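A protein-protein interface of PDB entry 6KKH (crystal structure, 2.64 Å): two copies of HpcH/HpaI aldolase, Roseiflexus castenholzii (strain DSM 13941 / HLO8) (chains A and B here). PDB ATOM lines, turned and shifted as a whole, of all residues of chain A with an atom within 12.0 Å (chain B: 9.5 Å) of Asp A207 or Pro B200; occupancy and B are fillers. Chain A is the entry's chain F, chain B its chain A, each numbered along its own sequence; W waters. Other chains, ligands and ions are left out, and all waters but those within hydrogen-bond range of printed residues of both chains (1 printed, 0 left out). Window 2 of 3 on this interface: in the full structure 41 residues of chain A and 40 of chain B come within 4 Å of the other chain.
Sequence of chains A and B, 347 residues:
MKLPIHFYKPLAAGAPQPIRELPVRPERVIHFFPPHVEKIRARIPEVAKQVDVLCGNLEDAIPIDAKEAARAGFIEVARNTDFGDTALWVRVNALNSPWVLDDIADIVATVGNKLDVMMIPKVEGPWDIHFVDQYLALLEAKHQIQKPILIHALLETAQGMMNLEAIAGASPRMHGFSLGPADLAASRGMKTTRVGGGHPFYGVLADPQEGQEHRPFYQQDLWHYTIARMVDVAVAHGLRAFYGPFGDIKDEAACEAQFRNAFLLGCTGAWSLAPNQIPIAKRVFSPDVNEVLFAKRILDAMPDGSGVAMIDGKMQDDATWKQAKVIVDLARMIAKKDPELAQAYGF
The backbone carbonyl oxygen of Gln B219 lies within hydrogen-bond range of the side-chain amide nitrogen of Gln A220, 2.7 Å away.
OE1 of Gln B220 lies close to OE1 of Gln A220 (2.9 Å).
N of Asp B221 lies within hydrogen-bond range of OE1 of Gln A220, 3.0 Å away.
The side-chain carboxylate (OD1) of Asp B251 lies within salt-bridge range of the guanidinium group (NH1) of Arg A215.
The backbone NH (N) of Val B204 is in hydrogen-bond range of the backbone carbonyl oxygen (O) of Tyr B218, 2.9 Å away.
OD1 of Asp B248 is in hydrogen-bond range of N of Asp B251.
The backbone carbonyl oxygen (O) of Val A204 is in hydrogen-bond range of the backbone NH (N) of Tyr A218, 2.9 Å away.
The backbone carbonyl oxygen (O) of Ala A206 sits at hydrogen-bond distance from the guanidinium group (NE) of Arg A215 (3.0 Å).
N of Ala A206 lies within hydrogen-bond range of O of Pro A216 (3.2 Å).
NE2 of Gln A220 is in hydrogen-bond range of O of Tyr A218 (3.4 Å).
CG2 of Val A204 touches C of Gln B220, 3.8 Å away.
N of Asp B221 touches CG2 of Val A204, at 3.7 Å.
Leu A205 touches Ala B254 (CD2 to N, 3.7 Å).
Gln B219 touches Ala A206 (NE2 to CB, 3.3 Å).
Pro B200 touches Asp A207.
CB of Ala B253 touches NH1 of Arg A215, 3.6 Å away.
CB of Ala B254 touches NH2 of Arg A215, 3.9 Å away.
Phe B217 touches Tyr A218 (O to CE2, 3.5 Å).
Tyr B218 touches Tyr A218 (CA to CD2, 3.7 Å).
Tyr A218 touches Gln B219 (CD2 to N, 3.7 Å).
Of chain B, only Gln B219 (3.3 Å) comes within 4 Å of Ala A206.
Of chain B, only Pro B200 (3.7 Å) comes within 4 Å of Asp A207.
No residue of chain B comes within 4 Å of Pro A208.
Phe A217 touches none of the printed residues of chain B.
Of the printed residues of chain B, Tyr A218 touches Phe B217 (3.5 Å), Tyr B218 (3.7 Å) and Gln B219 (3.7 Å).
Of the printed residues of chain B, Gln A220 touches Gln B219 (2.7 Å), Gln B220 (2.9 Å) and Asp B221 (3.0 Å).
No residue of chain A comes within 4 Å of Gly B198.
No residue of chain A comes within 4 Å of His B199.
Pro B200 touches just one residue of chain A: Asp A207 (3.7 Å).
No residue of chain A comes within 4 Å of Gly B203.
Of chain A, only Ala A206 (3.3 Å), Tyr A218 (3.7 Å) and Gln A220 (2.7 Å) come within 4 Å of Gln B219.
Of the printed residues of chain A, Ala B253 touches Leu A205 and Arg A215.
The nearest residue of chain A that does not touch Pro B200 is Ala A206 (6.6 Å).
Hydrophobic or aromatic side chains of chain A within 4 Å of the printed part of chain B: Val A204, Leu A205, Ala A206 and Tyr A218.
Among the printed residues, 15 pairs touch across the chains.
Val A204 touches Gln B220, but with the chains exchanged Gln A220 does not touch Val B204 (8.1 Å).
Tyr A218 touches Phe B217, but with the chains exchanged Phe A217 does not touch Tyr B218 (7.9 Å).
Tyr A218 touches its own counterpart, Tyr B218.
Gln B220 touches its own counterpart, Gln A220.
Of the 15 pairs that touch across the chains among the printed residues, 2 have their exchanged pair printed and touching as well.
Water W1 lies within hydrogen-bond range of OE1 of Gln B258 (3.3 Å) and N of Leu A205 (3.4 Å).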
ATOM      1  N   GLY A 203      -4.495  16.260  16.140  1.00  0.00           N
ATOM      2  CA  GLY A 203      -5.307  16.932  17.149  1.00  0.00           C
ATOM      3  C   GLY A 203      -5.759  18.312  16.714  1.00  0.00           C
ATOM      4  O   GLY A 203      -5.371  18.802  15.663  1.00  0.00           O
ATOM      5  N   VAL A 204      -6.587  18.915  17.556  1.00  0.00           N
ATOM      6  CA  VAL A 204      -7.159  20.237  17.336  1.00  0.00           C
ATOM      7  C   VAL A 204      -6.381  21.250  18.187  1.00  0.00           C
ATOM      8  O   VAL A 204      -6.083  20.993  19.355  1.00  0.00           O
ATOM      9  CB  VAL A 204      -8.663  20.245  17.684  1.00  0.00           C
ATOM     10  CG1 VAL A 204      -9.252  21.649  17.681  1.00  0.00           C
ATOM     11  CG2 VAL A 204      -9.458  19.327  16.766  1.00  0.00           C
ATOM     12  N   LEU A 205      -6.054  22.391  17.587  1.00  0.00           N
ATOM     13  CA  LEU A 205      -5.405  23.495  18.290  1.00  0.00           C
ATOM     14  C   LEU A 205      -6.466  24.543  18.638  1.00  0.00           C
ATOM     15  O   LEU A 205      -7.180  25.023  17.759  1.00  0.00           O
ATOM     16  CB  LEU A 205      -4.319  24.084  17.385  1.00  0.00           C
ATOM     17  CG  LEU A 205      -3.410  25.132  18.027  1.00  0.00           C
ATOM     18  CD1 LEU A 205      -2.490  24.498  19.062  1.00  0.00           C
ATOM     19  CD2 LEU A 205      -2.594  25.860  16.968  1.00  0.00           C
ATOM     20  N   ALA A 206      -6.561  24.901  19.915  1.00  0.00           N
ATOM     21  CA  ALA A 206      -7.628  25.796  20.374  1.00  0.00           C
ATOM     22  C   ALA A 206      -7.372  27.226  19.885  1.00  0.00           C
ATOM     23  O   ALA A 206      -6.273  27.555  19.425  1.00  0.00           O
ATOM     24  CB  ALA A 206      -7.725  25.745  21.878  1.00  0.00           C
ATOM     25  N   ASP A 207      -8.405  28.057  19.984  1.00  0.00           N
ATOM     26  CA  ASP A 207      -8.286  29.485  19.692  1.00  0.00           C
ATOM     27  C   ASP A 207      -7.407  30.135  20.771  1.00  0.00           C
ATOM     28  O   ASP A 207      -7.331  29.617  21.890  1.00  0.00           O
ATOM     29  CB  ASP A 207      -9.663  30.159  19.631  1.00  0.00           C
ATOM     30  CG  ASP A 207     -10.484  29.843  18.389  1.00  0.00           C
ATOM     31  OD1 ASP A 207      -9.918  29.261  17.441  1.00  0.00           O
ATOM     32  OD2 ASP A 207     -11.684  30.191  18.375  1.00  0.00           O
ATOM     33  N   PRO A 208      -6.730  31.261  20.441  1.00  0.00           N
ATOM     34  CA  PRO A 208      -6.044  32.078  21.459  1.00  0.00           C
ATOM     35  C   PRO A 208      -7.018  32.526  22.564  1.00  0.00           C
ATOM     36  O   PRO A 208      -8.183  32.813  22.279  1.00  0.00           O
ATOM     37  CB  PRO A 208      -5.486  33.285  20.694  1.00  0.00           C
ATOM     38  CG  PRO A 208      -5.294  32.760  19.299  1.00  0.00           C
ATOM     39  CD  PRO A 208      -6.452  31.806  19.103  1.00  0.00           C
ATOM     40  N   GLN A 209      -6.538  32.577  23.805  1.00  0.00           N
ATOM     41  CA  GLN A 209      -7.405  32.742  24.977  1.00  0.00           C
ATOM     42  C   GLN A 209      -7.204  34.140  25.576  1.00  0.00           C
ATOM     43  O   GLN A 209      -6.091  34.663  25.603  1.00  0.00           O
ATOM     44  CB  GLN A 209      -7.105  31.640  25.998  1.00  0.00           C
ATOM     45  CG  GLN A 209      -7.553  30.250  25.549  1.00  0.00           C
ATOM     46  CD  GLN A 209      -6.641  29.139  26.021  1.00  0.00           C
ATOM     47  OE1 GLN A 209      -5.465  29.078  25.664  1.00  0.00           O
ATOM     48  NE2 GLN A 209      -7.188  28.228  26.812  1.00  0.00           N
ATOM     49  N   ARG A 215      -1.590  27.713  23.924  1.00  0.00           N
ATOM     50  CA  ARG A 215      -2.646  27.177  23.051  1.00  0.00           C
ATOM     51  C   ARG A 215      -2.742  25.655  23.234  1.00  0.00           C
ATOM     52  O   ARG A 215      -1.880  24.908  22.742  1.00  0.00           O
ATOM     53  CB  ARG A 215      -2.373  27.531  21.585  1.00  0.00           C
ATOM     54  CG  ARG A 215      -2.856  28.916  21.183  1.00  0.00           C
ATOM     55  CD  ARG A 215      -2.564  29.253  19.730  1.00  0.00           C
ATOM     56  NE  ARG A 215      -3.700  29.036  18.838  1.00  0.00           N
ATOM     57  CZ  ARG A 215      -3.753  29.442  17.572  1.00  0.00           C
ATOM     58  NH1 ARG A 215      -2.682  29.955  16.989  1.00  0.00           N
ATOM     59  NH2 ARG A 215      -4.885  29.342  16.897  1.00  0.00           N
ATOM     60  N   PRO A 216      -3.789  25.189  23.937  1.00  0.00           N
ATOM     61  CA  PRO A 216      -4.020  23.757  24.183  1.00  0.00           C
ATOM     62  C   PRO A 216      -4.138  22.921  22.898  1.00  0.00           C
ATOM     63  O   PRO A 216      -4.518  23.430  21.841  1.00  0.00           O
ATOM     64  CB  PRO A 216      -5.350  23.701  24.949  1.00  0.00           C
ATOM     65  CG  PRO A 216      -5.450  25.050  25.615  1.00  0.00           C
ATOM     66  CD  PRO A 216      -4.787  26.001  24.644  1.00  0.00           C
ATOM     67  N   PHE A 217      -3.829  21.637  22.997  1.00  0.00           N
ATOM     68  CA  PHE A 217      -3.855  20.764  21.829  1.00  0.00           C
ATOM     69  C   PHE A 217      -4.544  19.444  22.191  1.00  0.00           C
ATOM     70  O   PHE A 217      -3.977  18.615  22.897  1.00  0.00           O
ATOM     71  CB  PHE A 217      -2.439  20.535  21.301  1.00  0.00           C
ATOM     72  CG  PHE A 217      -2.384  19.812  19.983  1.00  0.00           C
ATOM     73  CD1 PHE A 217      -2.674  20.477  18.802  1.00  0.00           C
ATOM     74  CD2 PHE A 217      -2.061  18.467  19.924  1.00  0.00           C
ATOM     75  CE1 PHE A 217      -2.629  19.815  17.586  1.00  0.00           C
ATOM     76  CE2 PHE A 217      -2.013  17.809  18.706  1.00  0.00           C
ATOM     77  CZ  PHE A 217      -2.296  18.483  17.540  1.00  0.00           C
ATOM     78  N   TYR A 218      -5.757  19.264  21.681  1.00  0.00           N
ATOM     79  CA  TYR A 218      -6.588  18.119  22.025  1.00  0.00           C
ATOM     80  C   TYR A 218      -6.426  17.026  20.959  1.00  0.00           C
ATOM     81  O   TYR A 218      -6.964  17.150  19.857  1.00  0.00           O
ATOM     82  CB  TYR A 218      -8.059  18.537  22.130  1.00  0.00           C
ATOM     83  CG  TYR A 218      -8.364  19.662  23.088  1.00  0.00           C
ATOM     84  CD1 TYR A 218      -8.138  20.985  22.739  1.00  0.00           C
ATOM     85  CD2 TYR A 218      -8.929  19.414  24.330  1.00  0.00           C
ATOM     86  CE1 TYR A 218      -8.436  22.025  23.606  1.00  0.00           C
ATOM     87  CE2 TYR A 218      -9.236  20.444  25.207  1.00  0.00           C
ATOM     88  CZ  TYR A 218      -8.990  21.755  24.844  1.00  0.00           C
ATOM     89  OH  TYR A 218      -9.286  22.778  25.697  1.00  0.00           O
ATOM     90  N   GLN A 220      -7.012  13.793  18.740  1.00  0.00           N
ATOM     91  CA  GLN A 220      -8.238  13.149  18.253  1.00  0.00           C
ATOM     92  C   GLN A 220      -7.923  11.690  17.901  1.00  0.00           C
ATOM     93  O   GLN A 220      -6.764  11.292  17.827  1.00  0.00           O
ATOM     94  CB  GLN A 220      -8.810  13.897  17.047  1.00  0.00           C
ATOM     95  CG  GLN A 220      -9.099  15.367  17.315  1.00  0.00           C
ATOM     96  CD  GLN A 220     -10.328  15.586  18.165  1.00  0.00           C
ATOM     97  OE1 GLN A 220     -11.443  15.237  17.783  1.00  0.00           O
ATOM     98  NE2 GLN A 220     -10.137  16.195  19.327  1.00  0.00           N
ATOM     99  N   LYS B 191     -21.196  24.799  10.574  1.00  0.00           N
ATOM    100  CA  LYS B 191     -20.740  26.135  11.009  1.00  0.00           C
ATOM    101  C   LYS B 191     -19.275  26.070  11.458  1.00  0.00           C
ATOM    102  O   LYS B 191     -18.895  25.251  12.303  1.00  0.00           O
ATOM    103  CB  LYS B 191     -21.626  26.695  12.126  1.00  0.00           C
ATOM    104  CG  LYS B 191     -23.045  27.062  11.706  1.00  0.00           C
ATOM    105  CD  LYS B 191     -24.020  25.925  11.919  1.00  0.00           C
ATOM    106  CE  LYS B 191     -25.426  26.219  11.441  1.00  0.00           C
ATOM    107  NZ  LYS B 191     -26.314  25.046  11.643  1.00  0.00           N
ATOM    108  N   THR B 192     -18.471  26.953  10.871  1.00  0.00           N
ATOM    109  CA  THR B 192     -17.050  27.064  11.178  1.00  0.00           C
ATOM    110  C   THR B 192     -16.694  28.544  11.332  1.00  0.00           C
ATOM    111  O   THR B 192     -17.388  29.406  10.795  1.00  0.00           O
ATOM    112  CB  THR B 192     -16.187  26.431  10.079  1.00  0.00           C
ATOM    113  OG1 THR B 192     -16.223  27.307   8.952  1.00  0.00           O
ATOM    114  CG2 THR B 192     -16.651  25.045   9.687  1.00  0.00           C
ATOM    115  N   THR B 193     -15.600  28.815  12.039  1.00  0.00           N
ATOM    116  CA  THR B 193     -15.202  30.185  12.367  1.00  0.00           C
ATOM    117  C   THR B 193     -14.139  30.680  11.375  1.00  0.00           C
ATOM    118  O   THR B 193     -13.909  31.880  11.270  1.00  0.00           O
ATOM    119  CB  THR B 193     -14.737  30.273  13.825  1.00  0.00           C
ATOM    120  OG1 THR B 193     -13.532  29.524  13.968  1.00  0.00           O
ATOM    121  CG2 THR B 193     -15.769  29.749  14.800  1.00  0.00           C
ATOM    122  N   ARG B 194     -13.494  29.766  10.660  1.00  0.00           N
ATOM    123  CA  ARG B 194     -12.517  30.124   9.637  1.00  0.00           C
ATOM    124  C   ARG B 194     -12.681  29.157   8.459  1.00  0.00           C
ATOM    125  O   ARG B 194     -13.050  28.004   8.657  1.00  0.00           O
ATOM    126  CB  ARG B 194     -11.095  30.051  10.206  1.00  0.00           C
ATOM    127  CG  ARG B 194     -10.850  30.927  11.429  1.00  0.00           C
ATOM    128  CD  ARG B 194     -10.694  32.405  11.098  1.00  0.00           C
ATOM    129  NE  ARG B 194     -11.345  33.295  12.054  1.00  0.00           N
ATOM    130  CZ  ARG B 194     -10.946  33.493  13.309  1.00  0.00           C
ATOM    131  NH1 ARG B 194      -9.944  32.794  13.816  1.00  0.00           N
ATOM    132  NH2 ARG B 194     -11.561  34.389  14.061  1.00  0.00           N
ATOM    133  N   GLY B 197     -11.262  25.615   8.698  1.00  0.00           N
ATOM    134  CA  GLY B 197     -11.003  25.399  10.120  1.00  0.00           C
ATOM    135  C   GLY B 197     -12.222  24.820  10.818  1.00  0.00           C
ATOM    136  O   GLY B 197     -13.257  24.606  10.194  1.00  0.00           O
ATOM    137  N   GLY B 198     -12.113  24.587  12.119  1.00  0.00           N
ATOM    138  CA  GLY B 198     -13.200  23.967  12.866  1.00  0.00           C
ATOM    139  C   GLY B 198     -14.058  24.993  13.585  1.00  0.00           C
ATOM    140  O   GLY B 198     -14.450  26.004  13.008  1.00  0.00           O
ATOM    141  N   HIS B 199     -14.348  24.710  14.852  1.00  0.00           N
ATOM    142  CA  HIS B 199     -15.180  25.572  15.677  1.00  0.00           C
ATOM    143  C   HIS B 199     -14.881  25.288  17.155  1.00  0.00           C
ATOM    144  O   HIS B 199     -14.893  24.128  17.571  1.00  0.00           O
ATOM    145  CB  HIS B 199     -16.655  25.350  15.340  1.00  0.00           C
ATOM    146  CG  HIS B 199     -17.572  26.428  15.807  1.00  0.00           C
ATOM    147  ND1 HIS B 199     -17.855  26.630  17.140  1.00  0.00           N
ATOM    148  CD2 HIS B 199     -18.303  27.333  15.125  1.00  0.00           C
ATOM    149  CE1 HIS B 199     -18.710  27.625  17.261  1.00  0.00           C
ATOM    150  NE2 HIS B 199     -19.002  28.073  16.038  1.00  0.00           N
ATOM    151  N   PRO B 200     -14.611  26.342  17.944  1.00  0.00           N
ATOM    152  CA  PRO B 200     -14.213  26.194  19.353  1.00  0.00           C
ATOM    153  C   PRO B 200     -15.265  25.483  20.223  1.00  0.00           C
ATOM    154  O   PRO B 200     -14.892  24.751  21.138  1.00  0.00           O
ATOM    155  CB  PRO B 200     -14.003  27.628  19.864  1.00  0.00           C
ATOM    156  CG  PRO B 200     -14.865  28.465  18.955  1.00  0.00           C
ATOM    157  CD  PRO B 200     -14.760  27.770  17.616  1.00  0.00           C
ATOM    158  N   PHE B 201     -16.551  25.694  19.927  1.00  0.00           N
ATOM    159  CA  PHE B 201     -17.651  25.139  20.721  1.00  0.00           C
ATOM    160  C   PHE B 201     -18.100  23.758  20.208  1.00  0.00           C
ATOM    161  O   PHE B 201     -19.149  23.267  20.644  1.00  0.00           O
ATOM    162  CB  PHE B 201     -18.856  26.087  20.710  1.00  0.00           C
ATOM    163  CG  PHE B 201     -18.629  27.471  21.271  1.00  0.00           C
ATOM    164  CD1 PHE B 201     -17.680  27.713  22.254  1.00  0.00           C
ATOM    165  CD2 PHE B 201     -19.414  28.533  20.844  1.00  0.00           C
ATOM    166  CE1 PHE B 201     -17.501  28.988  22.771  1.00  0.00           C
ATOM    167  CE2 PHE B 201     -19.234  29.806  21.363  1.00  0.00           C
ATOM    168  CZ  PHE B 201     -18.278  30.030  22.325  1.00  0.00           C
ATOM    169  N   TYR B 202     -17.356  23.124  19.295  1.00  0.00           N
ATOM    170  CA  TYR B 202     -17.643  21.728  18.922  1.00  0.00           C
ATOM    171  C   TYR B 202     -16.764  20.798  19.768  1.00  0.00           C
ATOM    172  O   TYR B 202     -15.570  20.636  19.508  1.00  0.00           O
ATOM    173  CB  TYR B 202     -17.443  21.481  17.421  1.00  0.00           C
ATOM    174  CG  TYR B 202     -17.665  20.047  17.001  1.00  0.00           C
ATOM    175  CD1 TYR B 202     -18.922  19.469  17.069  1.00  0.00           C
ATOM    176  CD2 TYR B 202     -16.618  19.252  16.563  1.00  0.00           C
ATOM    177  CE1 TYR B 202     -19.132  18.148  16.705  1.00  0.00           C
ATOM    178  CE2 TYR B 202     -16.811  17.933  16.184  1.00  0.00           C
ATOM    179  CZ  TYR B 202     -18.074  17.376  16.259  1.00  0.00           C
ATOM    180  OH  TYR B 202     -18.283  16.076  15.896  1.00  0.00           O
ATOM    181  N   GLY B 203     -17.361  20.182  20.778  1.00  0.00           N
ATOM    182  CA  GLY B 203     -16.586  19.360  21.708  1.00  0.00           C
ATOM    183  C   GLY B 203     -17.478  18.585  22.656  1.00  0.00           C
ATOM    184  O   GLY B 203     -18.694  18.752  22.636  1.00  0.00           O
ATOM    185  N   VAL B 204     -16.873  17.735  23.475  1.00  0.00           N
ATOM    186  CA  VAL B 204     -17.629  16.984  24.474  1.00  0.00           C
ATOM    187  C   VAL B 204     -17.389  17.617  25.850  1.00  0.00           C
ATOM    188  O   VAL B 204     -16.262  17.965  26.205  1.00  0.00           O
ATOM    189  CB  VAL B 204     -17.281  15.483  24.471  1.00  0.00           C
ATOM    190  CG1 VAL B 204     -17.489  14.862  23.096  1.00  0.00           C
ATOM    191  CG2 VAL B 204     -15.870  15.215  24.972  1.00  0.00           C
ATOM    192  N   PHE B 217     -13.852  20.678  28.793  1.00  0.00           N
ATOM    193  CA  PHE B 217     -14.467  20.636  27.470  1.00  0.00           C
ATOM    194  C   PHE B 217     -13.399  20.300  26.429  1.00  0.00           C
ATOM    195  O   PHE B 217     -12.548  21.129  26.123  1.00  0.00           O
ATOM    196  CB  PHE B 217     -15.139  21.975  27.167  1.00  0.00           C
ATOM    197  CG  PHE B 217     -15.948  22.012  25.895  1.00  0.00           C
ATOM    198  CD1 PHE B 217     -17.277  21.615  25.888  1.00  0.00           C
ATOM    199  CD2 PHE B 217     -15.389  22.469  24.711  1.00  0.00           C
ATOM    200  CE1 PHE B 217     -18.027  21.664  24.722  1.00  0.00           C
ATOM    201  CE2 PHE B 217     -16.140  22.514  23.545  1.00  0.00           C
ATOM    202  CZ  PHE B 217     -17.456  22.112  23.553  1.00  0.00           C
ATOM    203  N   TYR B 218     -13.454  19.079  25.902  1.00  0.00           N
ATOM    204  CA  TYR B 218     -12.480  18.610  24.918  1.00  0.00           C
ATOM    205  C   TYR B 218     -13.016  18.871  23.505  1.00  0.00           C
ATOM    206  O   TYR B 218     -14.049  18.311  23.115  1.00  0.00           O
ATOM    207  CB  TYR B 218     -12.184  17.120  25.107  1.00  0.00           C
ATOM    208  CG  TYR B 218     -11.793  16.712  26.505  1.00  0.00           C
ATOM    209  CD1 TYR B 218     -10.463  16.679  26.894  1.00  0.00           C
ATOM    210  CD2 TYR B 218     -12.750  16.330  27.432  1.00  0.00           C
ATOM    211  CE1 TYR B 218     -10.095  16.294  28.173  1.00  0.00           C
ATOM    212  CE2 TYR B 218     -12.398  15.939  28.714  1.00  0.00           C
ATOM    213  CZ  TYR B 218     -11.066  15.921  29.086  1.00  0.00           C
ATOM    214  OH  TYR B 218     -10.713  15.538  30.349  1.00  0.00           O
ATOM    215  N   GLN B 219     -12.299  19.708  22.752  1.00  0.00           N
ATOM    216  CA  GLN B 219     -12.696  20.090  21.394  1.00  0.00           C
ATOM    217  C   GLN B 219     -12.514  18.897  20.448  1.00  0.00           C
ATOM    218  O   GLN B 219     -11.529  18.151  20.551  1.00  0.00           O
ATOM    219  CB  GLN B 219     -11.884  21.295  20.913  1.00  0.00           C
ATOM    220  CG  GLN B 219     -12.224  22.586  21.647  1.00  0.00           C
ATOM    221  CD  GLN B 219     -11.620  23.803  20.986  1.00  0.00           C
ATOM    222  OE1 GLN B 219     -11.849  24.074  19.809  1.00  0.00           O
ATOM    223  NE2 GLN B 219     -10.836  24.549  21.748  1.00  0.00           N
ATOM    224  N   GLN B 220     -13.478  18.727  19.542  1.00  0.00           N
ATOM    225  CA  GLN B 220     -13.414  17.664  18.533  1.00  0.00           C
ATOM    226  C   GLN B 220     -13.139  18.290  17.159  1.00  0.00           C
ATOM    227  O   GLN B 220     -13.372  19.473  16.950  1.00  0.00           O
ATOM    228  CB  GLN B 220     -14.705  16.840  18.525  1.00  0.00           C
ATOM    229  CG  GLN B 220     -15.049  16.194  19.861  1.00  0.00           C
ATOM    230  CD  GLN B 220     -13.945  15.310  20.388  1.00  0.00           C
ATOM    231  OE1 GLN B 220     -13.477  14.393  19.716  1.00  0.00           O
ATOM    232  NE2 GLN B 220     -13.516  15.586  21.609  1.00  0.00           N
ATOM    233  N   ASP B 221     -12.623  17.475  16.244  1.00  0.00           N
ATOM    234  CA  ASP B 221     -12.332  17.892  14.876  1.00  0.00           C
ATOM    235  C   ASP B 221     -13.606  17.730  14.041  1.00  0.00           C
ATOM    236  O   ASP B 221     -14.225  16.668  14.049  1.00  0.00           O
ATOM    237  CB  ASP B 221     -11.173  17.080  14.293  1.00  0.00           C
ATOM    238  CG  ASP B 221     -10.924  17.309  12.814  1.00  0.00           C
ATOM    239  OD1 ASP B 221     -11.435  18.311  12.287  1.00  0.00           O
ATOM    240  OD2 ASP B 221     -10.217  16.476  12.196  1.00  0.00           O
ATOM    241  N   LEU B 222     -13.973  18.779  13.313  1.00  0.00           N
ATOM    242  CA  LEU B 222     -15.210  18.785  12.532  1.00  0.00           C
ATOM    243  C   LEU B 222     -15.033  18.011  11.219  1.00  0.00           C
ATOM    244  O   LEU B 222     -16.028  17.527  10.655  1.00  0.00           O
ATOM    245  CB  LEU B 222     -15.628  20.232  12.249  1.00  0.00           C
ATOM    246  CG  LEU B 222     -16.608  20.838  13.251  1.00  0.00           C
ATOM    247  CD1 LEU B 222     -16.735  22.336  13.039  1.00  0.00           C
ATOM    248  CD2 LEU B 222     -17.969  20.175  13.151  1.00  0.00           C
ATOM    249  N   PHE B 246      -6.660  26.868   3.727  1.00  0.00           N
ATOM    250  CA  PHE B 246      -6.906  27.409   5.048  1.00  0.00           C
ATOM    251  C   PHE B 246      -6.989  28.936   4.926  1.00  0.00           C
ATOM    252  O   PHE B 246      -6.094  29.561   4.363  1.00  0.00           O
ATOM    253  CB  PHE B 246      -5.809  26.949   6.005  1.00  0.00           C
ATOM    254  CG  PHE B 246      -6.063  27.290   7.447  1.00  0.00           C
ATOM    255  CD1 PHE B 246      -6.873  26.485   8.230  1.00  0.00           C
ATOM    256  CD2 PHE B 246      -5.490  28.415   8.020  1.00  0.00           C
ATOM    257  CE1 PHE B 246      -7.101  26.795   9.561  1.00  0.00           C
ATOM    258  CE2 PHE B 246      -5.724  28.726   9.350  1.00  0.00           C
ATOM    259  CZ  PHE B 246      -6.532  27.918  10.117  1.00  0.00           C
ATOM    260  N   ASP B 248      -7.484  31.602   7.280  1.00  0.00           N
ATOM    261  CA  ASP B 248      -6.862  32.534   8.251  1.00  0.00           C
ATOM    262  C   ASP B 248      -5.346  32.575   8.011  1.00  0.00           C
ATOM    263  O   ASP B 248      -4.586  31.806   8.611  1.00  0.00           O
ATOM    264  CB  ASP B 248      -7.209  32.131   9.689  1.00  0.00           C
ATOM    265  CG  ASP B 248      -6.876  33.159  10.762  1.00  0.00           C
ATOM    266  OD1 ASP B 248      -6.165  34.136  10.456  1.00  0.00           O
ATOM    267  OD2 ASP B 248      -7.325  32.963  11.910  1.00  0.00           O
ATOM    268  N   ASP B 251      -2.954  33.215  11.170  1.00  0.00           N
ATOM    269  CA  ASP B 251      -2.870  32.169  12.198  1.00  0.00           C
ATOM    270  C   ASP B 251      -2.081  30.970  11.653  1.00  0.00           C
ATOM    271  O   ASP B 251      -2.655  29.961  11.264  1.00  0.00           O
ATOM    272  CB  ASP B 251      -4.263  31.765  12.686  1.00  0.00           C
ATOM    273  CG  ASP B 251      -4.253  31.066  14.032  1.00  0.00           C
ATOM    274  OD1 ASP B 251      -3.193  30.521  14.397  1.00  0.00           O
ATOM    275  OD2 ASP B 251      -5.303  31.079  14.707  1.00  0.00           O
ATOM    276  N   ALA B 253      -0.072  28.890  13.182  1.00  0.00           N
ATOM    277  CA  ALA B 253      -0.004  27.707  14.044  1.00  0.00           C
ATOM    278  C   ALA B 253      -1.205  26.789  13.778  1.00  0.00           C
ATOM    279  O   ALA B 253      -1.060  25.568  13.781  1.00  0.00           O
ATOM    280  CB  ALA B 253       0.059  28.120  15.494  1.00  0.00           C
ATOM    281  N   ALA B 254      -2.380  27.385  13.566  1.00  0.00           N
ATOM    282  CA  ALA B 254      -3.609  26.636  13.263  1.00  0.00           C
ATOM    283  C   ALA B 254      -3.537  26.041  11.848  1.00  0.00           C
ATOM    284  O   ALA B 254      -4.064  24.958  11.590  1.00  0.00           O
ATOM    285  CB  ALA B 254      -4.809  27.540  13.415  1.00  0.00           C
ATOM    286  N   GLN B 258      -3.851  22.151  11.138  1.00  0.00           N
ATOM    287  CA  GLN B 258      -4.888  21.666  10.239  1.00  0.00           C
ATOM    288  C   GLN B 258      -4.250  20.865   9.095  1.00  0.00           C
ATOM    289  O   GLN B 258      -4.693  19.757   8.785  1.00  0.00           O
ATOM    290  CB  GLN B 258      -5.700  22.840   9.700  1.00  0.00           C
ATOM    291  CG  GLN B 258      -7.111  22.458   9.285  1.00  0.00           C
ATOM    292  CD  GLN B 258      -8.056  22.316  10.452  1.00  0.00           C
ATOM    293  OE1 GLN B 258      -7.657  22.315  11.615  1.00  0.00           O
ATOM    294  NE2 GLN B 258      -9.335  22.185  10.145  1.00  0.00           N
HETATM  295  O   HOH W   1      -6.368  23.499  14.394  1.00  0.00           O
